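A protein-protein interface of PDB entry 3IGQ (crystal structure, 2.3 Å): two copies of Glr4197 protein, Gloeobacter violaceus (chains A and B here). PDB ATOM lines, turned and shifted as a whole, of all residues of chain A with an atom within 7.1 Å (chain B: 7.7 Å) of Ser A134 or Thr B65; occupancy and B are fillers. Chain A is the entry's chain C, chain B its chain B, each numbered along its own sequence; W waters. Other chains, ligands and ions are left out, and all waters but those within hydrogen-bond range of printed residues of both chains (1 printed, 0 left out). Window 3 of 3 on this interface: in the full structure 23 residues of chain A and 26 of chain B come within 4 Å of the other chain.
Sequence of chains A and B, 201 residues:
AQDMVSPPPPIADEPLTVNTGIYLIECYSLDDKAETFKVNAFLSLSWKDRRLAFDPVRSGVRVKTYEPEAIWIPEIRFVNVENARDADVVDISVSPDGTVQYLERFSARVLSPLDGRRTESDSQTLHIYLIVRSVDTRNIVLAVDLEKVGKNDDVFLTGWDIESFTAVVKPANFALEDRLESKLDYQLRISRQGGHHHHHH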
ATOM      1  N   TRP A  72     -12.974 -20.338  27.088  1.00  0.00           N
ATOM      2  CA  TRP A  72     -11.743 -20.306  26.336  1.00  0.00           C
ATOM      3  C   TRP A  72     -12.008 -19.715  24.983  1.00  0.00           C
ATOM      4  O   TRP A  72     -13.032 -19.999  24.375  1.00  0.00           O
ATOM      5  CB  TRP A  72     -11.105 -21.698  26.237  1.00  0.00           C
ATOM      6  CG  TRP A  72      -9.813 -21.696  25.441  1.00  0.00           C
ATOM      7  CD1 TRP A  72      -8.552 -21.469  25.918  1.00  0.00           C
ATOM      8  CD2 TRP A  72      -9.675 -21.929  24.020  1.00  0.00           C
ATOM      9  NE1 TRP A  72      -7.649 -21.538  24.889  1.00  0.00           N
ATOM     10  CE2 TRP A  72      -8.302 -21.817  23.718  1.00  0.00           C
ATOM     11  CE3 TRP A  72     -10.589 -22.169  22.974  1.00  0.00           C
ATOM     12  CZ2 TRP A  72      -7.813 -21.972  22.431  1.00  0.00           C
ATOM     13  CZ3 TRP A  72     -10.109 -22.325  21.696  1.00  0.00           C
ATOM     14  CH2 TRP A  72      -8.733 -22.230  21.426  1.00  0.00           C
ATOM     15  N   GLU A  75      -6.506 -17.177  20.792  1.00  0.00           N
ATOM     16  CA  GLU A  75      -5.805 -15.907  20.810  1.00  0.00           C
ATOM     17  C   GLU A  75      -5.236 -15.657  19.427  1.00  0.00           C
ATOM     18  O   GLU A  75      -4.252 -16.292  19.019  1.00  0.00           O
ATOM     19  CB  GLU A  75      -4.692 -15.935  21.856  1.00  0.00           C
ATOM     20  CG  GLU A  75      -5.221 -16.277  23.246  1.00  0.00           C
ATOM     21  CD  GLU A  75      -4.265 -15.952  24.349  1.00  0.00           C
ATOM     22  OE1 GLU A  75      -3.649 -14.844  24.354  1.00  0.00           O
ATOM     23  OE2 GLU A  75      -4.149 -16.813  25.227  1.00  0.00           O
ATOM     24  N   VAL A 132      -2.475 -17.669  15.173  1.00  0.00           N
ATOM     25  CA  VAL A 132      -3.114 -17.991  16.433  1.00  0.00           C
ATOM     26  C   VAL A 132      -2.037 -18.557  17.361  1.00  0.00           C
ATOM     27  O   VAL A 132      -1.114 -19.239  16.902  1.00  0.00           O
ATOM     28  CB  VAL A 132      -4.270 -19.039  16.255  1.00  0.00           C
ATOM     29  CG1 VAL A 132      -3.742 -20.353  15.659  1.00  0.00           C
ATOM     30  CG2 VAL A 132      -5.057 -19.256  17.575  1.00  0.00           C
ATOM     31  N   ARG A 133      -2.137 -18.239  18.644  1.00  0.00           N
ATOM     32  CA  ARG A 133      -1.211 -18.790  19.635  1.00  0.00           C
ATOM     33  C   ARG A 133      -1.452 -20.277  19.869  1.00  0.00           C
ATOM     34  O   ARG A 133      -2.593 -20.776  19.863  1.00  0.00           O
ATOM     35  CB  ARG A 133      -1.300 -18.037  20.939  1.00  0.00           C
ATOM     36  CG  ARG A 133      -0.987 -16.547  20.822  1.00  0.00           C
ATOM     37  CD  ARG A 133      -0.745 -15.934  22.207  1.00  0.00           C
ATOM     38  NE  ARG A 133       0.179 -16.708  23.036  1.00  0.00           N
ATOM     39  CZ  ARG A 133       0.355 -16.567  24.348  1.00  0.00           C
ATOM     40  NH1 ARG A 133      -0.359 -15.691  25.051  1.00  0.00           N
ATOM     41  NH2 ARG A 133       1.244 -17.351  24.961  1.00  0.00           N
ATOM     42  N   SER A 134      -0.345 -20.990  20.021  1.00  0.00           N
ATOM     43  CA  SER A 134      -0.376 -22.408  20.315  1.00  0.00           C
ATOM     44  C   SER A 134      -0.824 -22.716  21.734  1.00  0.00           C
ATOM     45  O   SER A 134      -0.653 -21.912  22.642  1.00  0.00           O
ATOM     46  CB  SER A 134       0.994 -23.011  20.112  1.00  0.00           C
ATOM     47  OG  SER A 134       1.347 -22.954  18.751  1.00  0.00           O
ATOM     48  N   VAL A 135      -1.426 -23.889  21.884  1.00  0.00           N
ATOM     49  CA  VAL A 135      -1.734 -24.493  23.176  1.00  0.00           C
ATOM     50  C   VAL A 135      -1.198 -25.951  23.149  1.00  0.00           C
ATOM     51  O   VAL A 135      -1.052 -26.555  22.079  1.00  0.00           O
ATOM     52  CB  VAL A 135      -3.256 -24.453  23.467  1.00  0.00           C
ATOM     53  CG1 VAL A 135      -3.774 -23.043  23.491  1.00  0.00           C
ATOM     54  CG2 VAL A 135      -4.023 -25.277  22.448  1.00  0.00           C
ATOM     55  N   ASP A 136      -0.879 -26.541  24.297  1.00  0.00           N
ATOM     56  CA  ASP A 136      -0.214 -27.869  24.197  1.00  0.00           C
ATOM     57  C   ASP A 136      -1.175 -29.038  24.145  1.00  0.00           C
ATOM     58  O   ASP A 136      -0.821 -30.093  23.632  1.00  0.00           O
ATOM     59  CB  ASP A 136       0.900 -28.099  25.247  1.00  0.00           C
ATOM     60  CG  ASP A 136       0.441 -27.831  26.633  1.00  0.00           C
ATOM     61  OD1 ASP A 136      -0.779 -27.630  26.819  1.00  0.00           O
ATOM     62  OD2 ASP A 136       1.298 -27.815  27.531  1.00  0.00           O
ATOM     63  N   THR A 137      -2.394 -28.858  24.639  1.00  0.00           N
ATOM     64  CA  THR A 137      -3.373 -29.974  24.619  1.00  0.00           C
ATOM     65  C   THR A 137      -4.062 -30.151  23.259  1.00  0.00           C
ATOM     66  O   THR A 137      -4.631 -31.198  22.979  1.00  0.00           O
ATOM     67  CB  THR A 137      -4.408 -29.869  25.742  1.00  0.00           C
ATOM     68  OG1 THR A 137      -4.995 -28.551  25.716  1.00  0.00           O
ATOM     69  CG2 THR A 137      -3.730 -30.152  27.128  1.00  0.00           C
ATOM     70  N   ARG A 138      -3.995 -29.130  22.400  1.00  0.00           N
ATOM     71  CA  ARG A 138      -4.599 -29.204  21.049  1.00  0.00           C
ATOM     72  C   ARG A 138      -3.716 -28.630  19.953  1.00  0.00           C
ATOM     73  O   ARG A 138      -2.989 -27.645  20.138  1.00  0.00           O
ATOM     74  CB  ARG A 138      -5.912 -28.393  20.964  1.00  0.00           C
ATOM     75  CG  ARG A 138      -7.078 -28.784  21.869  1.00  0.00           C
ATOM     76  CD  ARG A 138      -7.666 -30.158  21.590  1.00  0.00           C
ATOM     77  NE  ARG A 138      -8.347 -30.367  20.327  1.00  0.00           N
ATOM     78  CZ  ARG A 138      -9.620 -30.117  20.047  1.00  0.00           C
ATOM     79  NH1 ARG A 138     -10.066 -30.460  18.852  1.00  0.00           N
ATOM     80  NH2 ARG A 138     -10.430 -29.558  20.932  1.00  0.00           N
ATOM     81  N   ASN A 139      -3.850 -29.195  18.778  1.00  0.00           N
ATOM     82  CA  ASN A 139      -3.358 -28.531  17.612  1.00  0.00           C
ATOM     83  C   ASN A 139      -4.403 -27.551  17.039  1.00  0.00           C
ATOM     84  O   ASN A 139      -5.468 -27.962  16.578  1.00  0.00           O
ATOM     85  CB  ASN A 139      -3.002 -29.576  16.576  1.00  0.00           C
ATOM     86  CG  ASN A 139      -2.504 -28.968  15.290  1.00  0.00           C
ATOM     87  OD1 ASN A 139      -2.796 -29.487  14.234  1.00  0.00           O
ATOM     88  ND2 ASN A 139      -1.753 -27.845  15.372  1.00  0.00           N
ATOM     89  N   ILE A 140      -4.109 -26.259  17.064  1.00  0.00           N
ATOM     90  CA  ILE A 140      -5.064 -25.292  16.589  1.00  0.00           C
ATOM     91  C   ILE A 140      -4.807 -24.969  15.109  1.00  0.00           C
ATOM     92  O   ILE A 140      -3.682 -24.646  14.697  1.00  0.00           O
ATOM     93  CB  ILE A 140      -5.146 -24.026  17.445  1.00  0.00           C
ATOM     94  CG1 ILE A 140      -5.428 -24.360  18.896  1.00  0.00           C
ATOM     95  CG2 ILE A 140      -6.247 -23.132  16.917  1.00  0.00           C
ATOM     96  CD1 ILE A 140      -5.339 -23.189  19.829  1.00  0.00           C
ATOM     97  N   ASP A 178       7.173 -22.590  14.015  1.00  0.00           N
ATOM     98  CA  ASP A 178       6.515 -22.611  15.328  1.00  0.00           C
ATOM     99  C   ASP A 178       5.351 -21.616  15.493  1.00  0.00           C
ATOM    100  O   ASP A 178       4.554 -21.759  16.422  1.00  0.00           O
ATOM    101  CB  ASP A 178       7.516 -22.560  16.518  1.00  0.00           C
ATOM    102  CG  ASP A 178       8.684 -21.541  16.332  1.00  0.00           C
ATOM    103  OD1 ASP A 178       9.547 -21.475  17.258  1.00  0.00           O
ATOM    104  OD2 ASP A 178       8.751 -20.825  15.294  1.00  0.00           O
ATOM    105  N   ARG A 179       5.279 -20.605  14.605  1.00  0.00           N
ATOM    106  CA  ARG A 179       4.121 -19.664  14.439  1.00  0.00           C
ATOM    107  C   ARG A 179       3.289 -20.363  13.424  1.00  0.00           C
ATOM    108  O   ARG A 179       2.477 -19.760  12.714  1.00  0.00           O
ATOM    109  CB  ARG A 179       4.512 -18.284  13.886  1.00  0.00           C
ATOM    110  N   LEU A 180       3.579 -21.659  13.346  1.00  0.00           N
ATOM    111  CA  LEU A 180       2.934 -22.609  12.469  1.00  0.00           C
ATOM    112  C   LEU A 180       2.145 -23.477  13.442  1.00  0.00           C
ATOM    113  O   LEU A 180       1.996 -24.725  13.231  1.00  0.00           O
ATOM    114  CB  LEU A 180       3.965 -23.409  11.612  1.00  0.00           C
ATOM    115  CG  LEU A 180       3.685 -24.064  10.215  1.00  0.00           C
ATOM    116  CD1 LEU A 180       3.532 -25.655  10.200  1.00  0.00           C
ATOM    117  CD2 LEU A 180       2.576 -23.361   9.342  1.00  0.00           C
ATOM    118  N   GLU A 181       1.633 -22.817  14.511  1.00  0.00           N
ATOM    119  CA  GLU A 181       0.309 -23.234  14.967  1.00  0.00           C
ATOM    120  C   GLU A 181      -0.517 -23.078  13.676  1.00  0.00           C
ATOM    121  O   GLU A 181      -0.820 -24.098  13.082  1.00  0.00           O
ATOM    122  CB  GLU A 181      -0.246 -22.524  16.213  1.00  0.00           C
ATOM    123  CG  GLU A 181      -1.438 -23.279  16.898  1.00  0.00           C
ATOM    124  CD  GLU A 181      -1.162 -24.754  17.414  1.00  0.00           C
ATOM    125  OE1 GLU A 181      -1.197 -25.731  16.630  1.00  0.00           O
ATOM    126  OE2 GLU A 181      -1.010 -24.956  18.641  1.00  0.00           O
ATOM    127  N   SER A 182      -0.733 -21.861  13.150  1.00  0.00           N
ATOM    128  CA  SER A 182      -1.509 -21.706  11.868  1.00  0.00           C
ATOM    129  C   SER A 182      -1.435 -20.271  11.264  1.00  0.00           C
ATOM    130  O   SER A 182      -1.386 -19.405  12.128  1.00  0.00           O
ATOM    131  CB  SER A 182      -2.968 -22.136  12.185  1.00  0.00           C
ATOM    132  OG  SER A 182      -3.618 -22.668  11.046  1.00  0.00           O
ATOM    133  N   PHE B  54      11.232 -33.648  29.640  1.00  0.00           N
ATOM    134  CA  PHE B  54      10.150 -34.584  29.943  1.00  0.00           C
ATOM    135  C   PHE B  54      10.250 -35.745  29.016  1.00  0.00           C
ATOM    136  O   PHE B  54      10.902 -35.658  27.990  1.00  0.00           O
ATOM    137  CB  PHE B  54       8.767 -33.897  29.838  1.00  0.00           C
ATOM    138  CG  PHE B  54       8.416 -33.379  28.440  1.00  0.00           C
ATOM    139  CD1 PHE B  54       8.754 -32.076  28.052  1.00  0.00           C
ATOM    140  CD2 PHE B  54       7.707 -34.174  27.560  1.00  0.00           C
ATOM    141  CE1 PHE B  54       8.411 -31.593  26.811  1.00  0.00           C
ATOM    142  CE2 PHE B  54       7.340 -33.684  26.299  1.00  0.00           C
ATOM    143  CZ  PHE B  54       7.708 -32.398  25.915  1.00  0.00           C
ATOM    144  N   VAL B  61       2.315 -35.905  25.584  1.00  0.00           N
ATOM    145  CA  VAL B  61       2.421 -34.798  24.645  1.00  0.00           C
ATOM    146  C   VAL B  61       3.859 -34.795  24.128  1.00  0.00           C
ATOM    147  O   VAL B  61       4.764 -35.268  24.819  1.00  0.00           O
ATOM    148  CB  VAL B  61       2.109 -33.416  25.294  1.00  0.00           C
ATOM    149  CG1 VAL B  61       0.637 -33.275  25.632  1.00  0.00           C
ATOM    150  CG2 VAL B  61       2.979 -33.169  26.518  1.00  0.00           C
ATOM    151  N   VAL B  63       5.327 -31.829  22.725  1.00  0.00           N
ATOM    152  CA  VAL B  63       5.805 -30.462  22.917  1.00  0.00           C
ATOM    153  C   VAL B  63       4.921 -29.906  24.025  1.00  0.00           C
ATOM    154  O   VAL B  63       3.738 -30.158  24.016  1.00  0.00           O
ATOM    155  CB  VAL B  63       5.658 -29.636  21.610  1.00  0.00           C
ATOM    156  CG1 VAL B  63       5.734 -28.160  21.864  1.00  0.00           C
ATOM    157  CG2 VAL B  63       6.742 -30.040  20.582  1.00  0.00           C
ATOM    158  N   LYS B  64       5.486 -29.190  24.987  1.00  0.00           N
ATOM    159  CA  LYS B  64       4.686 -28.522  26.010  1.00  0.00           C
ATOM    160  C   LYS B  64       4.664 -27.023  25.753  1.00  0.00           C
ATOM    161  O   LYS B  64       5.660 -26.455  25.329  1.00  0.00           O
ATOM    162  CB  LYS B  64       5.221 -28.786  27.413  1.00  0.00           C
ATOM    163  CG  LYS B  64       5.011 -30.201  27.845  1.00  0.00           C
ATOM    164  CD  LYS B  64       5.367 -30.374  29.277  1.00  0.00           C
ATOM    165  CE  LYS B  64       5.322 -31.848  29.659  1.00  0.00           C
ATOM    166  NZ  LYS B  64       5.211 -31.873  31.118  1.00  0.00           N
ATOM    167  N   THR B  65       3.523 -26.400  26.017  1.00  0.00           N
ATOM    168  CA  THR B  65       3.335 -24.979  25.839  1.00  0.00           C
ATOM    169  C   THR B  65       3.313 -24.299  27.201  1.00  0.00           C
ATOM    170  O   THR B  65       2.773 -24.831  28.183  1.00  0.00           O
ATOM    171  CB  THR B  65       2.039 -24.725  24.981  1.00  0.00           C
ATOM    172  OG1 THR B  65       2.228 -25.240  23.641  1.00  0.00           O
ATOM    173  CG2 THR B  65       1.723 -23.283  24.867  1.00  0.00           C
ATOM    174  N   TYR B  66       3.961 -23.147  27.283  1.00  0.00           N
ATOM    175  CA  TYR B  66       4.005 -22.416  28.551  1.00  0.00           C
ATOM    176  C   TYR B  66       3.602 -20.976  28.375  1.00  0.00           C
ATOM    177  O   TYR B  66       3.577 -20.415  27.283  1.00  0.00           O
ATOM    178  CB  TYR B  66       5.395 -22.489  29.210  1.00  0.00           C
ATOM    179  CG  TYR B  66       5.731 -23.820  29.874  1.00  0.00           C
ATOM    180  CD1 TYR B  66       6.250 -24.876  29.125  1.00  0.00           C
ATOM    181  CD2 TYR B  66       5.526 -24.020  31.246  1.00  0.00           C
ATOM    182  CE1 TYR B  66       6.553 -26.078  29.704  1.00  0.00           C
ATOM    183  CE2 TYR B  66       5.829 -25.250  31.850  1.00  0.00           C
ATOM    184  CZ  TYR B  66       6.341 -26.270  31.062  1.00  0.00           C
ATOM    185  OH  TYR B  66       6.645 -27.476  31.624  1.00  0.00           O
ATOM    186  N   GLU B  67       3.299 -20.358  29.492  1.00  0.00           N
ATOM    187  CA  GLU B  67       2.916 -18.984  29.511  1.00  0.00           C
ATOM    188  C   GLU B  67       4.165 -18.322  30.098  1.00  0.00           C
ATOM    189  O   GLU B  67       4.790 -18.914  31.013  1.00  0.00           O
ATOM    190  CB  GLU B  67       1.691 -18.870  30.440  1.00  0.00           C
ATOM    191  CG  GLU B  67       0.750 -17.739  30.116  1.00  0.00           C
ATOM    192  CD  GLU B  67      -0.099 -17.966  28.866  1.00  0.00           C
ATOM    193  OE1 GLU B  67      -0.799 -17.007  28.495  1.00  0.00           O
ATOM    194  OE2 GLU B  67      -0.087 -19.071  28.262  1.00  0.00           O
ATOM    195  N   PRO B  68       4.533 -17.110  29.599  1.00  0.00           N
ATOM    196  CA  PRO B  68       5.776 -16.433  30.014  1.00  0.00           C
ATOM    197  C   PRO B  68       5.965 -16.254  31.514  1.00  0.00           C
ATOM    198  O   PRO B  68       7.118 -16.240  31.987  1.00  0.00           O
ATOM    199  CB  PRO B  68       5.714 -15.056  29.333  1.00  0.00           C
ATOM    200  CG  PRO B  68       4.414 -14.994  28.628  1.00  0.00           C
ATOM    201  CD  PRO B  68       3.842 -16.383  28.526  1.00  0.00           C
ATOM    202  N   ALA B  70       5.158 -18.476  33.772  1.00  0.00           N
ATOM    203  CA  ALA B  70       5.419 -19.774  34.381  1.00  0.00           C
ATOM    204  C   ALA B  70       6.868 -20.297  34.233  1.00  0.00           C
ATOM    205  O   ALA B  70       7.212 -21.326  34.842  1.00  0.00           O
ATOM    206  CB  ALA B  70       4.440 -20.805  33.821  1.00  0.00           C
ATOM    207  N   ILE B  71       7.694 -19.659  33.399  1.00  0.00           N
ATOM    208  CA  ILE B  71       9.085 -20.088  33.207  1.00  0.00           C
ATOM    209  C   ILE B  71      10.069 -18.925  33.107  1.00  0.00           C
ATOM    210  O   ILE B  71       9.667 -17.774  32.865  1.00  0.00           O
ATOM    211  CB  ILE B  71       9.260 -20.981  32.002  1.00  0.00           C
ATOM    212  CG1 ILE B  71       8.896 -20.268  30.687  1.00  0.00           C
ATOM    213  CG2 ILE B  71       8.363 -22.211  32.132  1.00  0.00           C
ATOM    214  CD1 ILE B  71       9.396 -21.053  29.446  1.00  0.00           C
ATOM    215  N   VAL B  90       4.014 -14.860  21.128  1.00  0.00           N
ATOM    216  CA  VAL B  90       3.196 -15.657  20.219  1.00  0.00           C
ATOM    217  C   VAL B  90       3.232 -17.128  20.662  1.00  0.00           C
ATOM    218  O   VAL B  90       2.196 -17.832  20.695  1.00  0.00           O
ATOM    219  CB  VAL B  90       3.725 -15.554  18.764  1.00  0.00           C
ATOM    220  CG1 VAL B  90       3.055 -16.573  17.866  1.00  0.00           C
ATOM    221  CG2 VAL B  90       3.533 -14.147  18.215  1.00  0.00           C
ATOM    222  N   ASP B  91       4.423 -17.616  20.991  1.00  0.00           N
ATOM    223  CA  ASP B  91       4.602 -19.031  21.251  1.00  0.00           C
ATOM    224  C   ASP B  91       5.767 -19.278  22.165  1.00  0.00           C
ATOM    225  O   ASP B  91       6.831 -18.736  21.966  1.00  0.00           O
ATOM    226  CB  ASP B  91       4.843 -19.786  19.942  1.00  0.00           C
ATOM    227  CG  ASP B  91       4.847 -21.296  20.139  1.00  0.00           C
ATOM    228  OD1 ASP B  91       3.752 -21.854  20.339  1.00  0.00           O
ATOM    229  OD2 ASP B  91       5.944 -21.919  20.116  1.00  0.00           O
ATOM    230  N   ILE B  92       5.546 -20.092  23.183  1.00  0.00           N
ATOM    231  CA  ILE B  92       6.623 -20.651  23.985  1.00  0.00           C
ATOM    232  C   ILE B  92       6.408 -22.134  23.966  1.00  0.00           C
ATOM    233  O   ILE B  92       5.392 -22.652  24.423  1.00  0.00           O
ATOM    234  CB  ILE B  92       6.616 -20.170  25.423  1.00  0.00           C
ATOM    235  CG1 ILE B  92       6.789 -18.661  25.496  1.00  0.00           C
ATOM    236  CG2 ILE B  92       7.743 -20.841  26.188  1.00  0.00           C
ATOM    237  CD1 ILE B  92       6.621 -18.136  26.852  1.00  0.00           C
ATOM    238  N   SER B  93       7.347 -22.868  23.418  1.00  0.00           N
ATOM    239  CA  SER B  93       7.145 -24.292  23.430  1.00  0.00           C
ATOM    240  C   SER B  93       8.436 -25.058  23.784  1.00  0.00           C
ATOM    241  O   SER B  93       9.523 -24.681  23.397  1.00  0.00           O
ATOM    242  CB  SER B  93       6.506 -24.704  22.117  1.00  0.00           C
ATOM    243  OG  SER B  93       7.465 -24.649  21.129  1.00  0.00           O
ATOM    244  N   VAL B  94       8.299 -26.133  24.549  1.00  0.00           N
ATOM    245  CA  VAL B  94       9.426 -26.833  25.098  1.00  0.00           C
ATOM    246  C   VAL B  94       9.498 -28.251  24.541  1.00  0.00           C
ATOM    247  O   VAL B  94       8.510 -28.953  24.492  1.00  0.00           O
ATOM    248  CB  VAL B  94       9.323 -26.916  26.616  1.00  0.00           C
ATOM    249  CG1 VAL B  94      10.511 -27.653  27.184  1.00  0.00           C
ATOM    250  CG2 VAL B  94       9.187 -25.509  27.208  1.00  0.00           C
HETATM  251  O   HOH W   1       2.113 -27.286  29.903  1.00  0.00           O
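Printed residues of chain A that touch a printed residue of chain B: Arg A133, Ser A134, Val A135, Asp A136 and Asp A178.
Of the 15 printed residues of chain B, 6 touch a printed residue of chain A.
Among the printed residues, 9 pairs touch across the chains.
Among the printed residues, Asp or Glu carboxylates within 4 Å of a Lys or Arg side-chain nitrogen of the other chain: Arg A133 with Glu B67.
The backbone carbonyl oxygen (O) of Val B90 sits at hydrogen-bond distance from the guanidinium group (NE) of Arg A133, 3.3 Å away.
OE1 of Glu B67 lies within salt-bridge range of NH1 of Arg A133.
The side-chain carboxylate (OD2) of Asp A136 sits at hydrogen-bond distance from the backbone NH (N) of Thr B65 (3.0 Å).
The side-chain carboxylate (OD1) of Asp B91 lies close to the side-chain hydroxyl (OG) of Ser A134 (3.1 Å).
The side-chain carboxylate (OE1) of Glu A75 lies within salt-bridge range of the guanidinium group (NH1) of Arg A133 (3.5 Å).
The side-chain hydroxyl (OG) of Ser B93 is in hydrogen-bond range of the side-chain carboxylate (OD2) of Asp B91, at 3.3 Å.
The backbone carbonyl oxygen (O) of Lys B64 lies within hydrogen-bond range of the backbone NH (N) of Val B94, at 2.8 Å.
The backbone NH of Val A135 lies within hydrogen-bond range of the side-chain carboxylate of Glu A181, 3.4 Å away.
OG of Ser A134 lies close to OE2 of Glu A181 (3.1 Å).
Thr B65 touches Ser A134 (CG2 to O, 3.5 Å).
Val A135 touches Thr B65.
Asp A136 touches Val B63 (CB to O, 3.7 Å).
Lys B64 touches Asp A136 (CA to OD2, 3.8 Å).
O of Asp A178 touches CG of Asp B91 (3.8 Å).
Of chain B, only Thr B65 and Asp B91 come within 4 Å of Ser A134.
Printed residues of chain A within 4 Å of Val B63: Asp A136.
Of the printed residues of chain A, Thr B65 touches Ser A134 (3.5 Å), Val A135 (3.5 Å) and Asp A136 (3.0 Å).
Of the printed residues of chain A, Val B90 touches Arg A133 (3.3 Å).
The nearest printed residue of chain A that does not touch Thr B65 is Arg A133 (6.0 Å).
The nearest printed residue of chain A that does not touch Val B90 is Ser A134 (4.1 Å).
No position is printed for both chains.
Water W1 bridges the side-chain carboxylate of Asp A136 (2.6 Å) and the backbone carbonyl oxygen of Thr B65 (3.1 Å).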
